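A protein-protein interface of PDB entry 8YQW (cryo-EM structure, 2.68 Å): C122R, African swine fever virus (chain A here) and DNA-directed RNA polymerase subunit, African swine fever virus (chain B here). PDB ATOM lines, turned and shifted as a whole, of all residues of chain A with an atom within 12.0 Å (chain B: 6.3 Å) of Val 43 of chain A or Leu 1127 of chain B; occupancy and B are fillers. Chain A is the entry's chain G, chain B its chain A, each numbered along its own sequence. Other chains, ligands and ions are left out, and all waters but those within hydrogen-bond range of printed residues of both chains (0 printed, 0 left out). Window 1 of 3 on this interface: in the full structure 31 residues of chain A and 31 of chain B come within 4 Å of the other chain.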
ATOM      1  N   LEU A  38      10.679  44.083  21.063  1.00  0.00           N
ATOM      2  CA  LEU A  38      11.398  42.841  20.777  1.00  0.00           C
ATOM      3  C   LEU A  38      12.781  42.995  21.392  1.00  0.00           C
ATOM      4  O   LEU A  38      13.701  43.520  20.758  1.00  0.00           O
ATOM      5  CB  LEU A  38      11.466  42.558  19.281  1.00  0.00           C
ATOM      6  CG  LEU A  38      12.213  41.281  18.887  1.00  0.00           C
ATOM      7  CD1 LEU A  38      11.467  40.054  19.371  1.00  0.00           C
ATOM      8  CD2 LEU A  38      12.434  41.216  17.387  1.00  0.00           C
ATOM      9  N   VAL A  39      12.923  42.543  22.637  1.00  0.00           N
ATOM     10  CA  VAL A  39      14.179  42.729  23.354  1.00  0.00           C
ATOM     11  C   VAL A  39      15.272  41.853  22.757  1.00  0.00           C
ATOM     12  O   VAL A  39      16.395  42.310  22.521  1.00  0.00           O
ATOM     13  CB  VAL A  39      13.979  42.444  24.852  1.00  0.00           C
ATOM     14  CG1 VAL A  39      15.174  42.936  25.643  1.00  0.00           C
ATOM     15  CG2 VAL A  39      12.696  43.093  25.337  1.00  0.00           C
ATOM     16  N   SER A  40      14.961  40.586  22.500  1.00  0.00           N
ATOM     17  CA  SER A  40      15.958  39.654  21.996  1.00  0.00           C
ATOM     18  C   SER A  40      15.250  38.499  21.310  1.00  0.00           C
ATOM     19  O   SER A  40      14.044  38.300  21.475  1.00  0.00           O
ATOM     20  CB  SER A  40      16.864  39.141  23.120  1.00  0.00           C
ATOM     21  OG  SER A  40      18.015  38.502  22.597  1.00  0.00           O
ATOM     22  N   SER A  41      16.018  37.741  20.534  1.00  0.00           N
ATOM     23  CA  SER A  41      15.472  36.589  19.833  1.00  0.00           C
ATOM     24  C   SER A  41      16.605  35.639  19.477  1.00  0.00           C
ATOM     25  O   SER A  41      17.782  36.006  19.510  1.00  0.00           O
ATOM     26  CB  SER A  41      14.706  37.006  18.574  1.00  0.00           C
ATOM     27  OG  SER A  41      15.583  37.513  17.584  1.00  0.00           O
ATOM     28  N   LYS A  42      16.227  34.408  19.150  1.00  0.00           N
ATOM     29  CA  LYS A  42      17.157  33.426  18.614  1.00  0.00           C
ATOM     30  C   LYS A  42      16.363  32.412  17.810  1.00  0.00           C
ATOM     31  O   LYS A  42      15.214  32.119  18.141  1.00  0.00           O
ATOM     32  CB  LYS A  42      17.952  32.724  19.720  1.00  0.00           C
ATOM     33  CG  LYS A  42      19.058  31.830  19.190  1.00  0.00           C
ATOM     34  CD  LYS A  42      19.958  31.311  20.291  1.00  0.00           C
ATOM     35  CE  LYS A  42      21.102  30.499  19.705  1.00  0.00           C
ATOM     36  NZ  LYS A  42      22.026  29.987  20.748  1.00  0.00           N
ATOM     37  N   VAL A  43      16.977  31.890  16.753  1.00  0.00           N
ATOM     38  CA  VAL A  43      16.377  30.865  15.910  1.00  0.00           C
ATOM     39  C   VAL A  43      17.330  29.680  15.843  1.00  0.00           C
ATOM     40  O   VAL A  43      18.546  29.851  15.702  1.00  0.00           O
ATOM     41  CB  VAL A  43      16.039  31.408  14.504  1.00  0.00           C
ATOM     42  CG1 VAL A  43      17.285  31.912  13.801  1.00  0.00           C
ATOM     43  CG2 VAL A  43      15.338  30.346  13.671  1.00  0.00           C
ATOM     44  N   TYR A  44      16.780  28.479  15.977  1.00  0.00           N
ATOM     45  CA  TYR A  44      17.568  27.259  16.056  1.00  0.00           C
ATOM     46  C   TYR A  44      17.576  26.527  14.720  1.00  0.00           C
ATOM     47  O   TYR A  44      16.715  26.738  13.862  1.00  0.00           O
ATOM     48  CB  TYR A  44      17.029  26.345  17.158  1.00  0.00           C
ATOM     49  CG  TYR A  44      17.194  26.922  18.542  1.00  0.00           C
ATOM     50  CD1 TYR A  44      18.411  26.852  19.202  1.00  0.00           C
ATOM     51  CD2 TYR A  44      16.140  27.552  19.181  1.00  0.00           C
ATOM     52  CE1 TYR A  44      18.568  27.385  20.462  1.00  0.00           C
ATOM     53  CE2 TYR A  44      16.288  28.087  20.443  1.00  0.00           C
ATOM     54  CZ  TYR A  44      17.505  28.000  21.078  1.00  0.00           C
ATOM     55  OH  TYR A  44      17.661  28.531  22.336  1.00  0.00           O
ATOM     56  N   HIS A  45      18.573  25.656  14.559  1.00  0.00           N
ATOM     57  CA  HIS A  45      18.781  24.897  13.326  1.00  0.00           C
ATOM     58  C   HIS A  45      18.917  25.833  12.128  1.00  0.00           C
ATOM     59  O   HIS A  45      18.256  25.672  11.101  1.00  0.00           O
ATOM     60  CB  HIS A  45      17.659  23.878  13.104  1.00  0.00           C
ATOM     61  CG  HIS A  45      17.252  23.147  14.345  1.00  0.00           C
ATOM     62  ND1 HIS A  45      16.012  23.301  14.924  1.00  0.00           N
ATOM     63  CD2 HIS A  45      17.923  22.262  15.119  1.00  0.00           C
ATOM     64  CE1 HIS A  45      15.935  22.540  16.001  1.00  0.00           C
ATOM     65  NE2 HIS A  45      17.082  21.899  16.141  1.00  0.00           N
ATOM     66  N   THR A  46      19.787  26.834  12.276  1.00  0.00           N
ATOM     67  CA  THR A  46      20.013  27.795  11.205  1.00  0.00           C
ATOM     68  C   THR A  46      20.729  27.178  10.015  1.00  0.00           C
ATOM     69  O   THR A  46      20.590  27.680   8.895  1.00  0.00           O
ATOM     70  CB  THR A  46      20.817  28.986  11.723  1.00  0.00           C
ATOM     71  OG1 THR A  46      21.975  28.513  12.420  1.00  0.00           O
ATOM     72  CG2 THR A  46      19.977  29.816  12.669  1.00  0.00           C
ATOM     73  N   GLY A  47      21.481  26.103  10.227  1.00  0.00           N
ATOM     74  CA  GLY A  47      22.216  25.465   9.159  1.00  0.00           C
ATOM     75  C   GLY A  47      21.406  24.566   8.261  1.00  0.00           C
ATOM     76  O   GLY A  47      21.961  23.986   7.324  1.00  0.00           O
ATOM     77  N   GLU A  48      20.102  24.420   8.517  1.00  0.00           N
ATOM     78  CA  GLU A  48      19.269  23.568   7.678  1.00  0.00           C
ATOM     79  C   GLU A  48      17.890  24.168   7.415  1.00  0.00           C
ATOM     80  O   GLU A  48      16.971  23.434   7.031  1.00  0.00           O
ATOM     81  CB  GLU A  48      19.117  22.180   8.307  1.00  0.00           C
ATOM     82  CG  GLU A  48      18.372  22.169   9.631  1.00  0.00           C
ATOM     83  CD  GLU A  48      18.421  20.818  10.315  1.00  0.00           C
ATOM     84  OE1 GLU A  48      19.174  19.941   9.846  1.00  0.00           O
ATOM     85  OE2 GLU A  48      17.703  20.630  11.319  1.00  0.00           O
ATOM     86  N   MET A  49      17.716  25.473   7.606  1.00  0.00           N
ATOM     87  CA  MET A  49      16.418  26.085   7.363  1.00  0.00           C
ATOM     88  C   MET A  49      16.238  26.392   5.879  1.00  0.00           C
ATOM     89  O   MET A  49      17.200  26.486   5.112  1.00  0.00           O
ATOM     90  CB  MET A  49      16.249  27.359   8.191  1.00  0.00           C
ATOM     91  CG  MET A  49      17.436  28.305   8.161  1.00  0.00           C
ATOM     92  SD  MET A  49      17.153  29.758   9.190  1.00  0.00           S
ATOM     93  CE  MET A  49      18.724  30.603   9.040  1.00  0.00           C
ATOM     94  N   GLU A  50      14.973  26.550   5.480  1.00  0.00           N
ATOM     95  CA  GLU A  50      14.656  26.787   4.075  1.00  0.00           C
ATOM     96  C   GLU A  50      15.208  28.120   3.586  1.00  0.00           C
ATOM     97  O   GLU A  50      15.494  28.270   2.393  1.00  0.00           O
ATOM     98  CB  GLU A  50      13.142  26.725   3.866  1.00  0.00           C
ATOM     99  CG  GLU A  50      12.683  26.924   2.428  1.00  0.00           C
ATOM    100  CD  GLU A  50      13.108  25.794   1.512  1.00  0.00           C
ATOM    101  OE1 GLU A  50      13.255  24.653   1.998  1.00  0.00           O
ATOM    102  OE2 GLU A  50      13.298  26.049   0.304  1.00  0.00           O
ATOM    103  N   ASP A  51      15.372  29.091   4.483  1.00  0.00           N
ATOM    104  CA  ASP A  51      15.910  30.387   4.089  1.00  0.00           C
ATOM    105  C   ASP A  51      17.389  30.329   3.735  1.00  0.00           C
ATOM    106  O   ASP A  51      17.870  31.211   3.018  1.00  0.00           O
ATOM    107  CB  ASP A  51      15.679  31.405   5.206  1.00  0.00           C
ATOM    108  CG  ASP A  51      14.242  31.886   5.266  1.00  0.00           C
ATOM    109  OD1 ASP A  51      13.653  32.142   4.195  1.00  0.00           O
ATOM    110  OD2 ASP A  51      13.697  31.999   6.384  1.00  0.00           O
ATOM    111  N   LYS A  52      18.116  29.323   4.218  1.00  0.00           N
ATOM    112  CA  LYS A  52      19.526  29.166   3.886  1.00  0.00           C
ATOM    113  C   LYS A  52      19.749  28.622   2.485  1.00  0.00           C
ATOM    114  O   LYS A  52      20.681  29.058   1.800  1.00  0.00           O
ATOM    115  CB  LYS A  52      20.203  28.239   4.899  1.00  0.00           C
ATOM    116  CG  LYS A  52      21.577  27.769   4.470  1.00  0.00           C
ATOM    117  CD  LYS A  52      22.182  26.818   5.473  1.00  0.00           C
ATOM    118  CE  LYS A  52      23.442  26.188   4.918  1.00  0.00           C
ATOM    119  NZ  LYS A  52      24.048  25.232   5.882  1.00  0.00           N
ATOM    120  N   GLY A  87      19.844  18.669   5.024  1.00  0.00           N
ATOM    121  CA  GLY A  87      19.502  18.597   6.429  1.00  0.00           C
ATOM    122  C   GLY A  87      19.981  17.315   7.088  1.00  0.00           C
ATOM    123  O   GLY A  87      20.430  16.365   6.443  1.00  0.00           O
ATOM    124  N   SER A  88      19.881  17.307   8.418  1.00  0.00           N
ATOM    125  CA  SER A  88      20.199  16.117   9.197  1.00  0.00           C
ATOM    126  C   SER A  88      19.062  15.108   9.208  1.00  0.00           C
ATOM    127  O   SER A  88      19.274  13.963   9.619  1.00  0.00           O
ATOM    128  CB  SER A  88      20.557  16.499  10.634  1.00  0.00           C
ATOM    129  OG  SER A  88      19.410  16.915  11.353  1.00  0.00           O
ATOM    130  N   GLN A  89      17.868  15.502   8.779  1.00  0.00           N
ATOM    131  CA  GLN A  89      16.777  14.566   8.568  1.00  0.00           C
ATOM    132  C   GLN A  89      16.736  14.045   7.140  1.00  0.00           C
ATOM    133  O   GLN A  89      15.826  13.284   6.801  1.00  0.00           O
ATOM    134  CB  GLN A  89      15.439  15.217   8.925  1.00  0.00           C
ATOM    135  CG  GLN A  89      15.266  15.489  10.408  1.00  0.00           C
ATOM    136  CD  GLN A  89      15.253  14.219  11.238  1.00  0.00           C
ATOM    137  OE1 GLN A  89      14.574  13.250  10.900  1.00  0.00           O
ATOM    138  NE2 GLN A  89      16.010  14.217  12.328  1.00  0.00           N
ATOM    139  N   ILE A  91      16.189  15.492   4.016  1.00  0.00           N
ATOM    140  CA  ILE A  91      15.006  15.881   3.260  1.00  0.00           C
ATOM    141  C   ILE A  91      15.346  15.865   1.779  1.00  0.00           C
ATOM    142  O   ILE A  91      16.318  16.496   1.345  1.00  0.00           O
ATOM    143  CB  ILE A  91      14.506  17.265   3.703  1.00  0.00           C
ATOM    144  CG1 ILE A  91      14.119  17.246   5.183  1.00  0.00           C
ATOM    145  CG2 ILE A  91      13.331  17.701   2.853  1.00  0.00           C
ATOM    146  CD1 ILE A  91      12.953  16.339   5.498  1.00  0.00           C
ATOM    147  N   GLU B1123      15.226  23.440  25.511  1.00  0.00           N
ATOM    148  CA  GLU B1123      15.861  24.176  24.423  1.00  0.00           C
ATOM    149  C   GLU B1123      15.811  23.403  23.109  1.00  0.00           C
ATOM    150  O   GLU B1123      15.653  24.005  22.040  1.00  0.00           O
ATOM    151  CB  GLU B1123      17.303  24.508  24.799  1.00  0.00           C
ATOM    152  CG  GLU B1123      18.120  25.091  23.666  1.00  0.00           C
ATOM    153  CD  GLU B1123      19.431  25.676  24.142  1.00  0.00           C
ATOM    154  OE1 GLU B1123      19.660  25.697  25.370  1.00  0.00           O
ATOM    155  OE2 GLU B1123      20.231  26.118  23.292  1.00  0.00           O
ATOM    156  N   LEU B1125      13.569  21.454  21.941  1.00  0.00           N
ATOM    157  CA  LEU B1125      12.240  21.394  21.354  1.00  0.00           C
ATOM    158  C   LEU B1125      11.850  22.701  20.677  1.00  0.00           C
ATOM    159  O   LEU B1125      10.721  22.826  20.195  1.00  0.00           O
ATOM    160  CB  LEU B1125      11.208  21.033  22.422  1.00  0.00           C
ATOM    161  CG  LEU B1125      11.404  19.701  23.143  1.00  0.00           C
ATOM    162  CD1 LEU B1125      10.428  19.571  24.296  1.00  0.00           C
ATOM    163  CD2 LEU B1125      11.249  18.545  22.173  1.00  0.00           C
ATOM    164  N   ILE B1126      12.760  23.669  20.625  1.00  0.00           N
ATOM    165  CA  ILE B1126      12.466  25.028  20.192  1.00  0.00           C
ATOM    166  C   ILE B1126      13.064  25.256  18.811  1.00  0.00           C
ATOM    167  O   ILE B1126      14.207  24.863  18.548  1.00  0.00           O
ATOM    168  CB  ILE B1126      13.013  26.058  21.200  1.00  0.00           C
ATOM    169  CG1 ILE B1126      12.347  25.884  22.565  1.00  0.00           C
ATOM    170  CG2 ILE B1126      12.808  27.469  20.698  1.00  0.00           C
ATOM    171  CD1 ILE B1126      10.847  25.776  22.505  1.00  0.00           C
ATOM    172  N   LEU B1127      12.283  25.874  17.923  1.00  0.00           N
ATOM    173  CA  LEU B1127      12.828  26.411  16.682  1.00  0.00           C
ATOM    174  C   LEU B1127      13.331  27.837  16.861  1.00  0.00           C
ATOM    175  O   LEU B1127      14.436  28.168  16.420  1.00  0.00           O
ATOM    176  CB  LEU B1127      11.787  26.364  15.560  1.00  0.00           C
ATOM    177  CG  LEU B1127      11.540  25.022  14.877  1.00  0.00           C
ATOM    178  CD1 LEU B1127      10.409  25.135  13.879  1.00  0.00           C
ATOM    179  CD2 LEU B1127      12.807  24.539  14.197  1.00  0.00           C
ATOM    180  N   GLN B1128      12.537  28.691  17.503  1.00  0.00           N
ATOM    181  CA  GLN B1128      12.946  30.065  17.738  1.00  0.00           C
ATOM    182  C   GLN B1128      12.210  30.615  18.948  1.00  0.00           C
ATOM    183  O   GLN B1128      11.081  30.213  19.239  1.00  0.00           O
ATOM    184  CB  GLN B1128      12.682  30.942  16.513  1.00  0.00           C
ATOM    185  CG  GLN B1128      11.278  30.840  15.965  1.00  0.00           C
ATOM    186  CD  GLN B1128      11.097  31.681  14.725  1.00  0.00           C
ATOM    187  OE1 GLN B1128      12.050  32.271  14.220  1.00  0.00           O
ATOM    188  NE2 GLN B1128       9.872  31.737  14.219  1.00  0.00           N
ATOM    189  N   TRP B1129      12.858  31.547  19.644  1.00  0.00           N
ATOM    190  CA  TRP B1129      12.243  32.226  20.773  1.00  0.00           C
ATOM    191  C   TRP B1129      12.433  33.730  20.645  1.00  0.00           C
ATOM    192  O   TRP B1129      13.423  34.203  20.082  1.00  0.00           O
ATOM    193  CB  TRP B1129      12.809  31.740  22.116  1.00  0.00           C
ATOM    194  CG  TRP B1129      14.267  31.976  22.352  1.00  0.00           C
ATOM    195  CD1 TRP B1129      15.287  31.098  22.138  1.00  0.00           C
ATOM    196  CD2 TRP B1129      14.864  33.158  22.900  1.00  0.00           C
ATOM    197  NE1 TRP B1129      16.484  31.665  22.499  1.00  0.00           N
ATOM    198  CE2 TRP B1129      16.251  32.930  22.968  1.00  0.00           C
ATOM    199  CE3 TRP B1129      14.361  34.390  23.326  1.00  0.00           C
ATOM    200  CZ2 TRP B1129      17.140  33.889  23.447  1.00  0.00           C
ATOM    201  CZ3 TRP B1129      15.240  35.337  23.797  1.00  0.00           C
ATOM    202  CH2 TRP B1129      16.615  35.084  23.856  1.00  0.00           C
ATOM    203  N   GLU B1179       8.334  28.978  19.725  1.00  0.00           N
ATOM    204  CA  GLU B1179       7.775  28.278  18.572  1.00  0.00           C
ATOM    205  C   GLU B1179       8.360  26.870  18.581  1.00  0.00           C
ATOM    206  O   GLU B1179       9.532  26.674  18.247  1.00  0.00           O
ATOM    207  CB  GLU B1179       8.081  29.030  17.281  1.00  0.00           C
ATOM    208  CG  GLU B1179       7.145  28.718  16.128  1.00  0.00           C
ATOM    209  CD  GLU B1179       7.723  27.708  15.162  1.00  0.00           C
ATOM    210  OE1 GLU B1179       8.960  27.676  15.009  1.00  0.00           O
ATOM    211  OE2 GLU B1179       6.943  26.949  14.550  1.00  0.00           O
ATOM    212  N   LEU B1180       7.545  25.896  18.977  1.00  0.00           N
ATOM    213  CA  LEU B1180       8.028  24.535  19.159  1.00  0.00           C
ATOM    214  C   LEU B1180       8.341  23.878  17.821  1.00  0.00           C
ATOM    215  O   LEU B1180       7.648  24.092  16.824  1.00  0.00           O
ATOM    216  CB  LEU B1180       6.988  23.709  19.914  1.00  0.00           C
ATOM    217  CG  LEU B1180       6.890  23.914  21.426  1.00  0.00           C
ATOM    218  CD1 LEU B1180       5.672  23.204  21.976  1.00  0.00           C
ATOM    219  CD2 LEU B1180       8.144  23.415  22.110  1.00  0.00           C
ATOM    220  N   ASN B1181       9.400  23.070  17.804  1.00  0.00           N
ATOM    221  CA  ASN B1181       9.749  22.271  16.636  1.00  0.00           C
ATOM    222  C   ASN B1181       8.859  21.035  16.618  1.00  0.00           C
ATOM    223  O   ASN B1181       8.962  20.177  17.500  1.00  0.00           O
ATOM    224  CB  ASN B1181      11.226  21.888  16.678  1.00  0.00           C
ATOM    225  CG  ASN B1181      11.731  21.364  15.352  1.00  0.00           C
ATOM    226  OD1 ASN B1181      10.952  21.037  14.460  1.00  0.00           O
ATOM    227  ND2 ASN B1181      13.046  21.282  15.216  1.00  0.00           N
ATOM    228  N   LYS B1182       7.982  20.939  15.619  1.00  0.00           N
ATOM    229  CA  LYS B1182       7.037  19.831  15.578  1.00  0.00           C
ATOM    230  C   LYS B1182       7.692  18.519  15.173  1.00  0.00           C
ATOM    231  O   LYS B1182       7.221  17.456  15.589  1.00  0.00           O
ATOM    232  CB  LYS B1182       5.881  20.155  14.632  1.00  0.00           C
ATOM    233  CG  LYS B1182       4.894  21.157  15.204  1.00  0.00           C
ATOM    234  CD  LYS B1182       3.671  21.303  14.317  1.00  0.00           C
ATOM    235  CE  LYS B1182       3.967  22.148  13.093  1.00  0.00           C
ATOM    236  NZ  LYS B1182       2.738  22.394  12.294  1.00  0.00           N
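The backbone carbonyl oxygen (O) of Leu 1127 of chain B lies within hydrogen-bond range of the backbone NH (N) of Tyr 44 of chain A, 2.4 Å away. The backbone NH (N) of Trp 1129 of chain B lies within hydrogen-bond range of the backbone carbonyl oxygen (O) of Lys 42 of chain A, 2.9 Å away. The indole nitrogen (NE1) of Trp 1129 of chain B lies within hydrogen-bond range of the side-chain hydroxyl (OH) of Tyr 44 of chain A (3.4 Å).
The backbone carbonyl oxygen of Leu 1125 of chain B is in hydrogen-bond range of the backbone NH of Asn 1181 of chain B (2.7 Å). N of Leu 1127 of chain B is in hydrogen-bond range of O of Glu 1179 of chain B (2.9 Å). The backbone NH (N) of Glu 1179 of chain B sits at hydrogen-bond distance from the backbone carbonyl oxygen (O) of Gln 1128 of chain B (3.1 Å).
Among the printed residues, pairs that only touch across the chains: Ser 40 of chain A with Trp 1129 of chain B, Ser 41 of chain A with Trp 1129 of chain B, Lys 42 of chain A with Gln 1128 of chain B, Val 43 of chain A with Leu 1127 of chain B, Val 43 of chain A with Gln 1128 of chain B, Tyr 44 of chain A with Glu 1123 of chain B, Tyr 44 of chain A with Ile 1126 of chain B, His 45 of chain A with Ile 1126 of chain B, His 45 of chain A with Leu 1127 of chain B and His 45 of chain A with Asn 1181 of chain B.
Val 43 of chain A touches just these residues of chain B: Leu 1127 (3.3 Å) and Gln 1128 (3.7 Å). Printed residues of chain B within 4 Å of His 45 of chain A: Ile 1126 (3.9 Å), Leu 1127 (3.5 Å) and Asn 1181 (3.2 Å). Ile 1126 of chain B touches just these residues of chain A: Tyr 44 (3.4 Å) and His 45 (3.9 Å). Of chain A, only Val 43, Tyr 44 and His 45 come within 4 Å of Leu 1127 of chain B. Printed residues of chain A within 4 Å of Trp 1129 of chain B: Ser 40, Ser 41, Lys 42 and Tyr 44. No residue of chain A comes within 4 Å of Glu 1179 of chain B. Asn 1181 of chain B touches one residue of chain A. Lys 1182 of chain B touches none of the printed residues of chain A. The nearest residue of chain B that does not touch Val 43 of chain A is Trp 1129 of chain B (5.0 Å). The nearest residue of chain A that does not touch Leu 1127 of chain B is Lys 42 of chain A (4.4 Å). The nearest printed residue of chain B that does not touch Ser 41 of chain A is Gln 1128 of chain B (6.7 Å).
Hydrophobic or aromatic side chains of chain B that line the printed part of chain A: Ile 1126, Leu 1127 and Trp 1129. Of the 19 printed residues of chain A, 6 touch a printed residue of chain B. Among the printed residues, 13 pairs touch across the chains. Among the printed residues, no Asp or Glu carboxylate lies within 4 Å of a Lys or Arg side-chain nitrogen of the other chain.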
